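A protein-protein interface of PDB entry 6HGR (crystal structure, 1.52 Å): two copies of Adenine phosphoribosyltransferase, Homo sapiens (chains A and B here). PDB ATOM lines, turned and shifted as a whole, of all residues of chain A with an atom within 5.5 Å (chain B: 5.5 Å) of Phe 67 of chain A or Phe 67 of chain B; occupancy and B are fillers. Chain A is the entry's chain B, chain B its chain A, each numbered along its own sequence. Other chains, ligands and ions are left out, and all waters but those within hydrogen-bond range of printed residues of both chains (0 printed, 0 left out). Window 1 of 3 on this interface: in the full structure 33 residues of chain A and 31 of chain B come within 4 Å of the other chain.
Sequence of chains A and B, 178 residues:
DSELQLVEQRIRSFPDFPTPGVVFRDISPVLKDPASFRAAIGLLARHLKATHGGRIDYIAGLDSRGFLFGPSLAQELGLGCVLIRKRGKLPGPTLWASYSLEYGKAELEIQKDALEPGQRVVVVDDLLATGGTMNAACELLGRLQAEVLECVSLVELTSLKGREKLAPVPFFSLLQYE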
ATOM      1  N   GLY A  61     -27.273   9.386  -6.027  1.00  0.00           N
ATOM      2  CA  GLY A  61     -26.178  10.330  -6.038  1.00  0.00           C
ATOM      3  C   GLY A  61     -24.926   9.715  -5.448  1.00  0.00           C
ATOM      4  O   GLY A  61     -24.999   8.989  -4.437  1.00  0.00           O
ATOM      5  N   LEU A  62     -23.779  10.002  -6.061  1.00  0.00           N
ATOM      6  CA  LEU A  62     -22.508   9.434  -5.601  1.00  0.00           C
ATOM      7  C   LEU A  62     -21.718  10.400  -4.701  1.00  0.00           C
ATOM      8  O   LEU A  62     -21.512  11.559  -5.047  1.00  0.00           O
ATOM      9  CB  LEU A  62     -21.646   9.040  -6.797  1.00  0.00           C
ATOM     10  CG  LEU A  62     -22.264   8.056  -7.789  1.00  0.00           C
ATOM     11  CD1 LEU A  62     -21.200   7.441  -8.688  1.00  0.00           C
ATOM     12  CD2 LEU A  62     -23.086   6.988  -7.091  1.00  0.00           C
ATOM     13  N   ASP A  63     -21.298   9.906  -3.541  1.00  0.00           N
ATOM     14  CA  ASP A  63     -20.438  10.629  -2.584  1.00  0.00           C
ATOM     15  C   ASP A  63     -19.120  10.981  -3.277  1.00  0.00           C
ATOM     16  O   ASP A  63     -18.502  10.086  -3.843  1.00  0.00           O
ATOM     17  CB  ASP A  63     -20.140   9.641  -1.436  1.00  0.00           C
ATOM     18  CG  ASP A  63     -19.684  10.295  -0.129  1.00  0.00           C
ATOM     19  OD1 ASP A  63     -19.454  11.520  -0.068  1.00  0.00           O
ATOM     20  OD2 ASP A  63     -19.553   9.535   0.872  1.00  0.00           O
ATOM     21  N   SER A  64     -18.660  12.237  -3.258  1.00  0.00           N
ATOM     22  CA  SER A  64     -19.311  13.335  -2.563  1.00  0.00           C
ATOM     23  C   SER A  64     -19.895  14.376  -3.529  1.00  0.00           C
ATOM     24  O   SER A  64     -20.877  15.057  -3.217  1.00  0.00           O
ATOM     25  CB  SER A  64     -18.299  14.020  -1.641  1.00  0.00           C
ATOM     26  OG  SER A  64     -18.817  15.233  -1.139  1.00  0.00           O
ATOM     27  N   ARG A  65     -19.289  14.538  -4.703  1.00  0.00           N
ATOM     28  CA  ARG A  65     -19.745  15.641  -5.575  1.00  0.00           C
ATOM     29  C   ARG A  65     -21.036  15.326  -6.330  1.00  0.00           C
ATOM     30  O   ARG A  65     -21.740  16.229  -6.781  1.00  0.00           O
ATOM     31  CB  ARG A  65     -18.624  16.094  -6.512  1.00  0.00           C
ATOM     32  CG  ARG A  65     -17.509  16.822  -5.780  1.00  0.00           C
ATOM     33  CD  ARG A  65     -16.520  17.459  -6.745  1.00  0.00           C
ATOM     34  NE  ARG A  65     -15.598  16.473  -7.306  1.00  0.00           N
ATOM     35  CZ  ARG A  65     -14.363  16.264  -6.854  1.00  0.00           C
ATOM     36  NH1 ARG A  65     -13.891  16.985  -5.842  1.00  0.00           N
ATOM     37  NH2 ARG A  65     -13.594  15.345  -7.418  1.00  0.00           N
ATOM     38  N   GLY A  66     -21.401  14.054  -6.416  1.00  0.00           N
ATOM     39  CA  GLY A  66     -22.703  13.699  -6.933  1.00  0.00           C
ATOM     40  C   GLY A  66     -23.839  14.128  -6.012  1.00  0.00           C
ATOM     41  O   GLY A  66     -24.958  14.342  -6.461  1.00  0.00           O
ATOM     42  N   PHE A  67     -23.550  14.188  -4.716  1.00  0.00           N
ATOM     43  CA  PHE A  67     -24.475  14.694  -3.707  1.00  0.00           C
ATOM     44  C   PHE A  67     -24.894  16.125  -4.032  1.00  0.00           C
ATOM     45  O   PHE A  67     -25.966  16.552  -3.648  1.00  0.00           O
ATOM     46  CB  PHE A  67     -23.829  14.680  -2.323  1.00  0.00           C
ATOM     47  CG  PHE A  67     -23.728  13.319  -1.685  1.00  0.00           C
ATOM     48  CD1 PHE A  67     -24.073  12.172  -2.381  1.00  0.00           C
ATOM     49  CD2 PHE A  67     -23.247  13.206  -0.409  1.00  0.00           C
ATOM     50  CE1 PHE A  67     -23.977  10.922  -1.789  1.00  0.00           C
ATOM     51  CE2 PHE A  67     -23.125  11.965   0.198  1.00  0.00           C
ATOM     52  CZ  PHE A  67     -23.496  10.823  -0.492  1.00  0.00           C
ATOM     53  N   LEU A  68     -24.043  16.862  -4.723  1.00  0.00           N
ATOM     54  CA  LEU A  68     -24.365  18.246  -5.076  1.00  0.00           C
ATOM     55  C   LEU A  68     -25.462  18.367  -6.116  1.00  0.00           C
ATOM     56  O   LEU A  68     -26.188  19.374  -6.170  1.00  0.00           O
ATOM     57  CB  LEU A  68     -23.117  18.945  -5.594  1.00  0.00           C
ATOM     58  CG  LEU A  68     -22.008  19.209  -4.594  1.00  0.00           C
ATOM     59  CD1 LEU A  68     -20.765  19.642  -5.347  1.00  0.00           C
ATOM     60  CD2 LEU A  68     -22.405  20.268  -3.576  1.00  0.00           C
ATOM     61  N   PHE A  69     -25.574  17.356  -6.960  1.00  0.00           N
ATOM     62  CA  PHE A  69     -26.513  17.402  -8.070  1.00  0.00           C
ATOM     63  C   PHE A  69     -27.695  16.472  -7.855  1.00  0.00           C
ATOM     64  O   PHE A  69     -28.772  16.750  -8.336  1.00  0.00           O
ATOM     65  CB  PHE A  69     -25.785  17.076  -9.373  1.00  0.00           C
ATOM     66  CG  PHE A  69     -24.693  18.048  -9.682  1.00  0.00           C
ATOM     67  CD1 PHE A  69     -24.994  19.289 -10.204  1.00  0.00           C
ATOM     68  CD2 PHE A  69     -23.379  17.779  -9.315  1.00  0.00           C
ATOM     69  CE1 PHE A  69     -24.009  20.233 -10.405  1.00  0.00           C
ATOM     70  CE2 PHE A  69     -22.397  18.723  -9.515  1.00  0.00           C
ATOM     71  CZ  PHE A  69     -22.708  19.942 -10.072  1.00  0.00           C
ATOM     72  N   GLY A  70     -27.487  15.369  -7.144  1.00  0.00           N
ATOM     73  CA  GLY A  70     -28.514  14.332  -7.030  1.00  0.00           C
ATOM     74  C   GLY A  70     -29.840  14.825  -6.494  1.00  0.00           C
ATOM     75  O   GLY A  70     -30.871  14.619  -7.116  1.00  0.00           O
ATOM     76  N   PRO A  71     -29.840  15.451  -5.306  1.00  0.00           N
ATOM     77  CA  PRO A  71     -31.119  15.893  -4.768  1.00  0.00           C
ATOM     78  C   PRO A  71     -31.827  16.935  -5.613  1.00  0.00           C
ATOM     79  O   PRO A  71     -33.031  16.835  -5.776  1.00  0.00           O
ATOM     80  CB  PRO A  71     -30.762  16.426  -3.368  1.00  0.00           C
ATOM     81  CG  PRO A  71     -29.515  15.728  -3.024  1.00  0.00           C
ATOM     82  CD  PRO A  71     -28.763  15.577  -4.314  1.00  0.00           C
ATOM     83  N   LEU A  83     -28.538   7.349  -1.729  1.00  0.00           N
ATOM     84  CA  LEU A  83     -27.152   7.723  -1.571  1.00  0.00           C
ATOM     85  C   LEU A  83     -26.232   6.516  -1.674  1.00  0.00           C
ATOM     86  O   LEU A  83     -26.468   5.476  -1.025  1.00  0.00           O
ATOM     87  CB  LEU A  83     -26.934   8.339  -0.194  1.00  0.00           C
ATOM     88  CG  LEU A  83     -27.835   9.521   0.156  1.00  0.00           C
ATOM     89  CD1 LEU A  83     -27.517  10.041   1.554  1.00  0.00           C
ATOM     90  CD2 LEU A  83     -27.665  10.604  -0.888  1.00  0.00           C
ATOM     91  N   ILE A  84     -25.158   6.675  -2.439  1.00  0.00           N
ATOM     92  CA  ILE A  84     -24.071   5.706  -2.440  1.00  0.00           C
ATOM     93  C   ILE A  84     -22.860   6.404  -1.822  1.00  0.00           C
ATOM     94  O   ILE A  84     -22.433   7.441  -2.306  1.00  0.00           O
ATOM     95  CB  ILE A  84     -23.800   5.187  -3.846  1.00  0.00           C
ATOM     96  CG1 ILE A  84     -25.021   4.369  -4.321  1.00  0.00           C
ATOM     97  CG2 ILE A  84     -22.507   4.389  -3.886  1.00  0.00           C
ATOM     98  CD1 ILE A  84     -24.967   3.901  -5.754  1.00  0.00           C
ATOM     99  N   ARG A  85     -22.381   5.890  -0.700  1.00  0.00           N
ATOM    100  CA  ARG A  85     -21.405   6.589   0.121  1.00  0.00           C
ATOM    101  C   ARG A  85     -20.066   5.895   0.119  1.00  0.00           C
ATOM    102  O   ARG A  85     -19.972   4.707  -0.168  1.00  0.00           O
ATOM    103  CB  ARG A  85     -21.897   6.664   1.563  1.00  0.00           C
ATOM    104  CG  ARG A  85     -23.175   7.461   1.744  1.00  0.00           C
ATOM    105  CD  ARG A  85     -23.025   8.430   2.898  1.00  0.00           C
ATOM    106  NE  ARG A  85     -21.799   9.205   2.747  1.00  0.00           N
ATOM    107  CZ  ARG A  85     -21.300  10.021   3.671  1.00  0.00           C
ATOM    108  NH1 ARG A  85     -21.912  10.168   4.837  1.00  0.00           N
ATOM    109  NH2 ARG A  85     -20.177  10.686   3.425  1.00  0.00           N
ATOM    110  N   GLY B  61     -21.785  24.976   1.819  1.00  0.00           N
ATOM    111  CA  GLY B  61     -22.136  23.596   2.126  1.00  0.00           C
ATOM    112  C   GLY B  61     -20.926  22.837   2.623  1.00  0.00           C
ATOM    113  O   GLY B  61     -19.844  22.956   2.050  1.00  0.00           O
ATOM    114  N   LEU B  62     -21.099  22.050   3.686  1.00  0.00           N
ATOM    115  CA  LEU B  62     -20.016  21.215   4.218  1.00  0.00           C
ATOM    116  C   LEU B  62     -19.982  19.800   3.625  1.00  0.00           C
ATOM    117  O   LEU B  62     -20.992  19.084   3.591  1.00  0.00           O
ATOM    118  CB  LEU B  62     -20.108  21.100   5.736  1.00  0.00           C
ATOM    119  CG  LEU B  62     -20.070  22.434   6.480  1.00  0.00           C
ATOM    120  CD1 LEU B  62     -19.814  22.245   7.970  1.00  0.00           C
ATOM    121  CD2 LEU B  62     -19.037  23.369   5.867  1.00  0.00           C
ATOM    122  N   ASP B  63     -18.812  19.410   3.147  1.00  0.00           N
ATOM    123  CA  ASP B  63     -18.547  18.032   2.732  1.00  0.00           C
ATOM    124  C   ASP B  63     -18.798  17.081   3.899  1.00  0.00           C
ATOM    125  O   ASP B  63     -18.316  17.360   5.001  1.00  0.00           O
ATOM    126  CB  ASP B  63     -17.063  17.956   2.363  1.00  0.00           C
ATOM    127  CG  ASP B  63     -16.720  16.797   1.455  1.00  0.00           C
ATOM    128  OD1 ASP B  63     -17.577  15.917   1.228  1.00  0.00           O
ATOM    129  OD2 ASP B  63     -15.564  16.783   0.965  1.00  0.00           O
ATOM    130  N   SER B  64     -19.549  15.983   3.714  1.00  0.00           N
ATOM    131  CA  SER B  64     -20.208  15.642   2.459  1.00  0.00           C
ATOM    132  C   SER B  64     -21.733  15.753   2.543  1.00  0.00           C
ATOM    133  O   SER B  64     -22.415  15.910   1.528  1.00  0.00           O
ATOM    134  CB  SER B  64     -19.845  14.207   2.064  1.00  0.00           C
ATOM    135  OG  SER B  64     -20.190  13.957   0.718  1.00  0.00           O
ATOM    136  N   ARG B  65     -22.295  15.602   3.741  1.00  0.00           N
ATOM    137  CA  ARG B  65     -23.756  15.589   3.818  1.00  0.00           C
ATOM    138  C   ARG B  65     -24.352  17.000   3.747  1.00  0.00           C
ATOM    139  O   ARG B  65     -25.513  17.151   3.401  1.00  0.00           O
ATOM    140  CB  ARG B  65     -24.267  14.801   5.025  1.00  0.00           C
ATOM    141  CG  ARG B  65     -24.141  13.292   4.864  1.00  0.00           C
ATOM    142  CD  ARG B  65     -24.837  12.536   5.992  1.00  0.00           C
ATOM    143  NE  ARG B  65     -24.026  12.477   7.210  1.00  0.00           N
ATOM    144  CZ  ARG B  65     -23.472  11.367   7.695  1.00  0.00           C
ATOM    145  NH1 ARG B  65     -23.645  10.202   7.083  1.00  0.00           N
ATOM    146  NH2 ARG B  65     -22.746  11.420   8.804  1.00  0.00           N
ATOM    147  N   GLY B  66     -23.539  18.027   3.984  1.00  0.00           N
ATOM    148  CA  GLY B  66     -23.952  19.389   3.711  1.00  0.00           C
ATOM    149  C   GLY B  66     -24.201  19.629   2.233  1.00  0.00           C
ATOM    150  O   GLY B  66     -24.983  20.506   1.854  1.00  0.00           O
ATOM    151  N   PHE B  67     -23.474  18.891   1.399  1.00  0.00           N
ATOM    152  CA  PHE B  67     -23.563  19.006  -0.050  1.00  0.00           C
ATOM    153  C   PHE B  67     -24.952  18.584  -0.516  1.00  0.00           C
ATOM    154  O   PHE B  67     -25.391  18.988  -1.581  1.00  0.00           O
ATOM    155  CB  PHE B  67     -22.526  18.094  -0.735  1.00  0.00           C
ATOM    156  CG  PHE B  67     -21.100  18.621  -0.740  1.00  0.00           C
ATOM    157  CD1 PHE B  67     -20.724  19.740  -0.011  1.00  0.00           C
ATOM    158  CD2 PHE B  67     -20.135  17.951  -1.460  1.00  0.00           C
ATOM    159  CE1 PHE B  67     -19.417  20.207  -0.052  1.00  0.00           C
ATOM    160  CE2 PHE B  67     -18.825  18.396  -1.487  1.00  0.00           C
ATOM    161  CZ  PHE B  67     -18.466  19.532  -0.783  1.00  0.00           C
ATOM    162  N   LEU B  68     -25.637  17.756   0.268  1.00  0.00           N
ATOM    163  CA  LEU B  68     -26.978  17.305  -0.101  1.00  0.00           C
ATOM    164  C   LEU B  68     -28.025  18.397   0.022  1.00  0.00           C
ATOM    165  O   LEU B  68     -29.068  18.362  -0.659  1.00  0.00           O
ATOM    166  CB  LEU B  68     -27.386  16.139   0.786  1.00  0.00           C
ATOM    167  CG  LEU B  68     -26.620  14.849   0.563  1.00  0.00           C
ATOM    168  CD1 LEU B  68     -26.845  13.927   1.755  1.00  0.00           C
ATOM    169  CD2 LEU B  68     -27.050  14.187  -0.732  1.00  0.00           C
ATOM    170  N   PHE B  69     -27.795  19.317   0.952  1.00  0.00           N
ATOM    171  CA  PHE B  69     -28.766  20.361   1.257  1.00  0.00           C
ATOM    172  C   PHE B  69     -28.338  21.722   0.755  1.00  0.00           C
ATOM    173  O   PHE B  69     -29.187  22.525   0.389  1.00  0.00           O
ATOM    174  CB  PHE B  69     -29.028  20.395   2.766  1.00  0.00           C
ATOM    175  CG  PHE B  69     -29.602  19.111   3.282  1.00  0.00           C
ATOM    176  CD1 PHE B  69     -30.946  18.842   3.124  1.00  0.00           C
ATOM    177  CD2 PHE B  69     -28.784  18.121   3.790  1.00  0.00           C
ATOM    178  CE1 PHE B  69     -31.492  17.646   3.537  1.00  0.00           C
ATOM    179  CE2 PHE B  69     -29.318  16.919   4.188  1.00  0.00           C
ATOM    180  CZ  PHE B  69     -30.675  16.678   4.065  1.00  0.00           C
ATOM    181  N   GLY B  70     -27.041  21.986   0.727  1.00  0.00           N
ATOM    182  CA  GLY B  70     -26.557  23.333   0.386  1.00  0.00           C
ATOM    183  C   GLY B  70     -27.069  23.879  -0.934  1.00  0.00           C
ATOM    184  O   GLY B  70     -27.604  24.991  -0.991  1.00  0.00           O
ATOM    185  N   PRO B  71     -26.871  23.140  -2.033  1.00  0.00           N
ATOM    186  CA  PRO B  71     -27.318  23.636  -3.327  1.00  0.00           C
ATOM    187  C   PRO B  71     -28.820  23.865  -3.438  1.00  0.00           C
ATOM    188  O   PRO B  71     -29.247  24.869  -4.000  1.00  0.00           O
ATOM    189  CB  PRO B  71     -26.852  22.547  -4.297  1.00  0.00           C
ATOM    190  CG  PRO B  71     -25.708  21.924  -3.618  1.00  0.00           C
ATOM    191  CD  PRO B  71     -26.067  21.917  -2.171  1.00  0.00           C
ATOM    192  N   LEU B  83     -18.267  25.713  -1.444  1.00  0.00           N
ATOM    193  CA  LEU B  83     -18.034  24.385  -0.908  1.00  0.00           C
ATOM    194  C   LEU B  83     -16.867  24.384   0.037  1.00  0.00           C
ATOM    195  O   LEU B  83     -15.795  24.914  -0.276  1.00  0.00           O
ATOM    196  CB  LEU B  83     -17.740  23.405  -2.053  1.00  0.00           C
ATOM    197  CG  LEU B  83     -18.814  23.391  -3.145  1.00  0.00           C
ATOM    198  CD1 LEU B  83     -18.407  22.488  -4.306  1.00  0.00           C
ATOM    199  CD2 LEU B  83     -20.137  22.968  -2.547  1.00  0.00           C
ATOM    200  N   ILE B  84     -17.065  23.749   1.185  1.00  0.00           N
ATOM    201  CA  ILE B  84     -15.979  23.457   2.086  1.00  0.00           C
ATOM    202  C   ILE B  84     -15.755  21.960   2.113  1.00  0.00           C
ATOM    203  O   ILE B  84     -16.688  21.210   2.362  1.00  0.00           O
ATOM    204  CB  ILE B  84     -16.289  23.968   3.487  1.00  0.00           C
ATOM    205  CG1 ILE B  84     -16.395  25.498   3.455  1.00  0.00           C
ATOM    206  CG2 ILE B  84     -15.231  23.479   4.471  1.00  0.00           C
ATOM    207  CD1 ILE B  84     -16.989  26.108   4.699  1.00  0.00           C
ATOM    208  N   ARG B  85     -14.556  21.550   1.720  1.00  0.00           N
ATOM    209  CA  ARG B  85     -14.253  20.143   1.449  1.00  0.00           C
ATOM    210  C   ARG B  85     -13.333  19.542   2.484  1.00  0.00           C
ATOM    211  O   ARG B  85     -12.588  20.250   3.154  1.00  0.00           O
ATOM    212  CB  ARG B  85     -13.578  20.021   0.082  1.00  0.00           C
ATOM    213  CG  ARG B  85     -14.494  20.393  -1.074  1.00  0.00           C
ATOM    214  CD  ARG B  85     -14.555  19.280  -2.107  1.00  0.00           C
ATOM    215  NE  ARG B  85     -14.903  18.006  -1.481  1.00  0.00           N
ATOM    216  CZ  ARG B  85     -14.877  16.828  -2.096  1.00  0.00           C
ATOM    217  NH1 ARG B  85     -14.502  16.741  -3.365  1.00  0.00           N
ATOM    218  NH2 ARG B  85     -15.202  15.734  -1.428  1.00  0.00           N
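NH1 of Arg 65 of chain A sits close to NH1 of Arg 85 of chain B, 2.6 Å away. The side-chain carboxylate of Asp 63 of chain B sits at hydrogen-bond distance from the side-chain hydroxyl of Ser 64 of chain A (2.8 Å). The side-chain hydroxyl (OG) of Ser 64 of chain A sits at hydrogen-bond distance from the side-chain hydroxyl (OG) of Ser 64 of chain B, 2.6 Å away. OG of Ser 64 of chain B sits at hydrogen-bond distance from OD1 of Asp 63 of chain A (2.7 Å). The guanidinium group of Arg 85 of chain A lies close to the guanidinium group of Arg 65 of chain B, at 2.8 Å. O of Phe 67 of chain B lies close to O of Phe 67 of chain A, at 3.2 Å.
O of Ile 84 of chain B is in hydrogen-bond range of N of Asp 63 of chain B, 2.9 Å away. The side-chain hydroxyl (OG) of Ser 64 of chain B sits close to the side-chain carboxylate (OD1) of Asp 63 of chain B, 3.3 Å away. The backbone carbonyl oxygen of Ile 84 of chain A sits at hydrogen-bond distance from the backbone NH of Asp 63 of chain A, at 3.0 Å. OD2 of Asp 63 of chain B is in salt-bridge range of NH2 of Arg 85 of chain B, 2.6 Å away. The side-chain carboxylate (OD2) of Asp 63 of chain A is in salt-bridge range of the guanidinium group (NH2) of Arg 85 of chain A (2.9 Å). The backbone NH (N) of Phe 67 of chain A is in hydrogen-bond range of the backbone carbonyl oxygen (O) of Leu 62 of chain A.
Among the printed residues, merely in contact across the chains: Ser 64 of chain A with Phe 67 of chain B, Phe 67 of chain A with Ser 64 of chain B, Leu 68 of chain A with Phe 67 of chain B, Ser 64 of chain A with Arg 85 of chain B, Phe 67 of chain A with Leu 68 of chain B, Pro 71 of chain A with Leu 68 of chain B, Leu 83 of chain A with Leu 68 of chain B, Leu 68 of chain A with Pro 71 of chain B, Leu 68 of chain A with Leu 83 of chain B and Arg 85 of chain A with Ser 64 of chain B.
Printed residues of chain A within 4 Å of Phe 67 of chain B: Ser 64 (3.0 Å), Phe 67 (3.2 Å) and Leu 68 (3.5 Å). Of the printed residues of chain B, Asp 63 of chain A touches Ser 64 (2.7 Å). Of the printed residues of chain A, Leu 68 of chain B touches Phe 67, Pro 71 and Leu 83. Of the printed residues of chain A, Arg 65 of chain B touches Arg 85 (2.8 Å). Printed residues of chain A within 4 Å of Leu 83 of chain B: Leu 68. Of the printed residues of chain B, Ser 64 of chain A touches Asp 63, Ser 64, Phe 67 and Arg 85. Gly 61 of chain B touches none of the printed residues of chain A. Phe 69 of chain A touches none of the printed residues of chain B. The nearest printed residue of chain B that does not touch Phe 67 of chain A is Arg 65 of chain B (4.9 Å). The nearest printed residue of chain A that does not touch Phe 67 of chain B is Arg 65 of chain A (4.7 Å).
Of the 14 printed residues of chain B, 8 touch a printed residue of chain A. Printed residues of chain B that touch a printed residue of chain A: Asp 63, Ser 64, Arg 65, Phe 67, Leu 68, Pro 71, Leu 83 and Arg 85. Of the 14 printed residues of chain A, 8 touch a printed residue of chain B. Hydrophobic or aromatic side chains of chain A that line the printed part of chain B: Phe 67, Leu 68, Pro 71 and Leu 83. Among the printed residues, 16 pairs touch across the chains. Among the printed residues, no Asp or Glu carboxylate lies within 4 Å of a Lys or Arg side-chain nitrogen of the other chain.
Ser 64 of chain B touches its own counterpart, Ser 64 of chain A. Arg 65 of chain A touches Arg 85 of chain B, and with the chains exchanged Arg 85 of chain A touches Arg 65 of chain B. Phe 67 of chain A touches its own counterpart, Phe 67 of chain B. Leu 68 of chain A touches Leu 83 of chain B, and with the chains exchanged Leu 83 of chain A touches Leu 68 of chain B. Of the 16 pairs that touch across the chains among the printed residues, 16 have their exchanged pair printed and touching as well.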
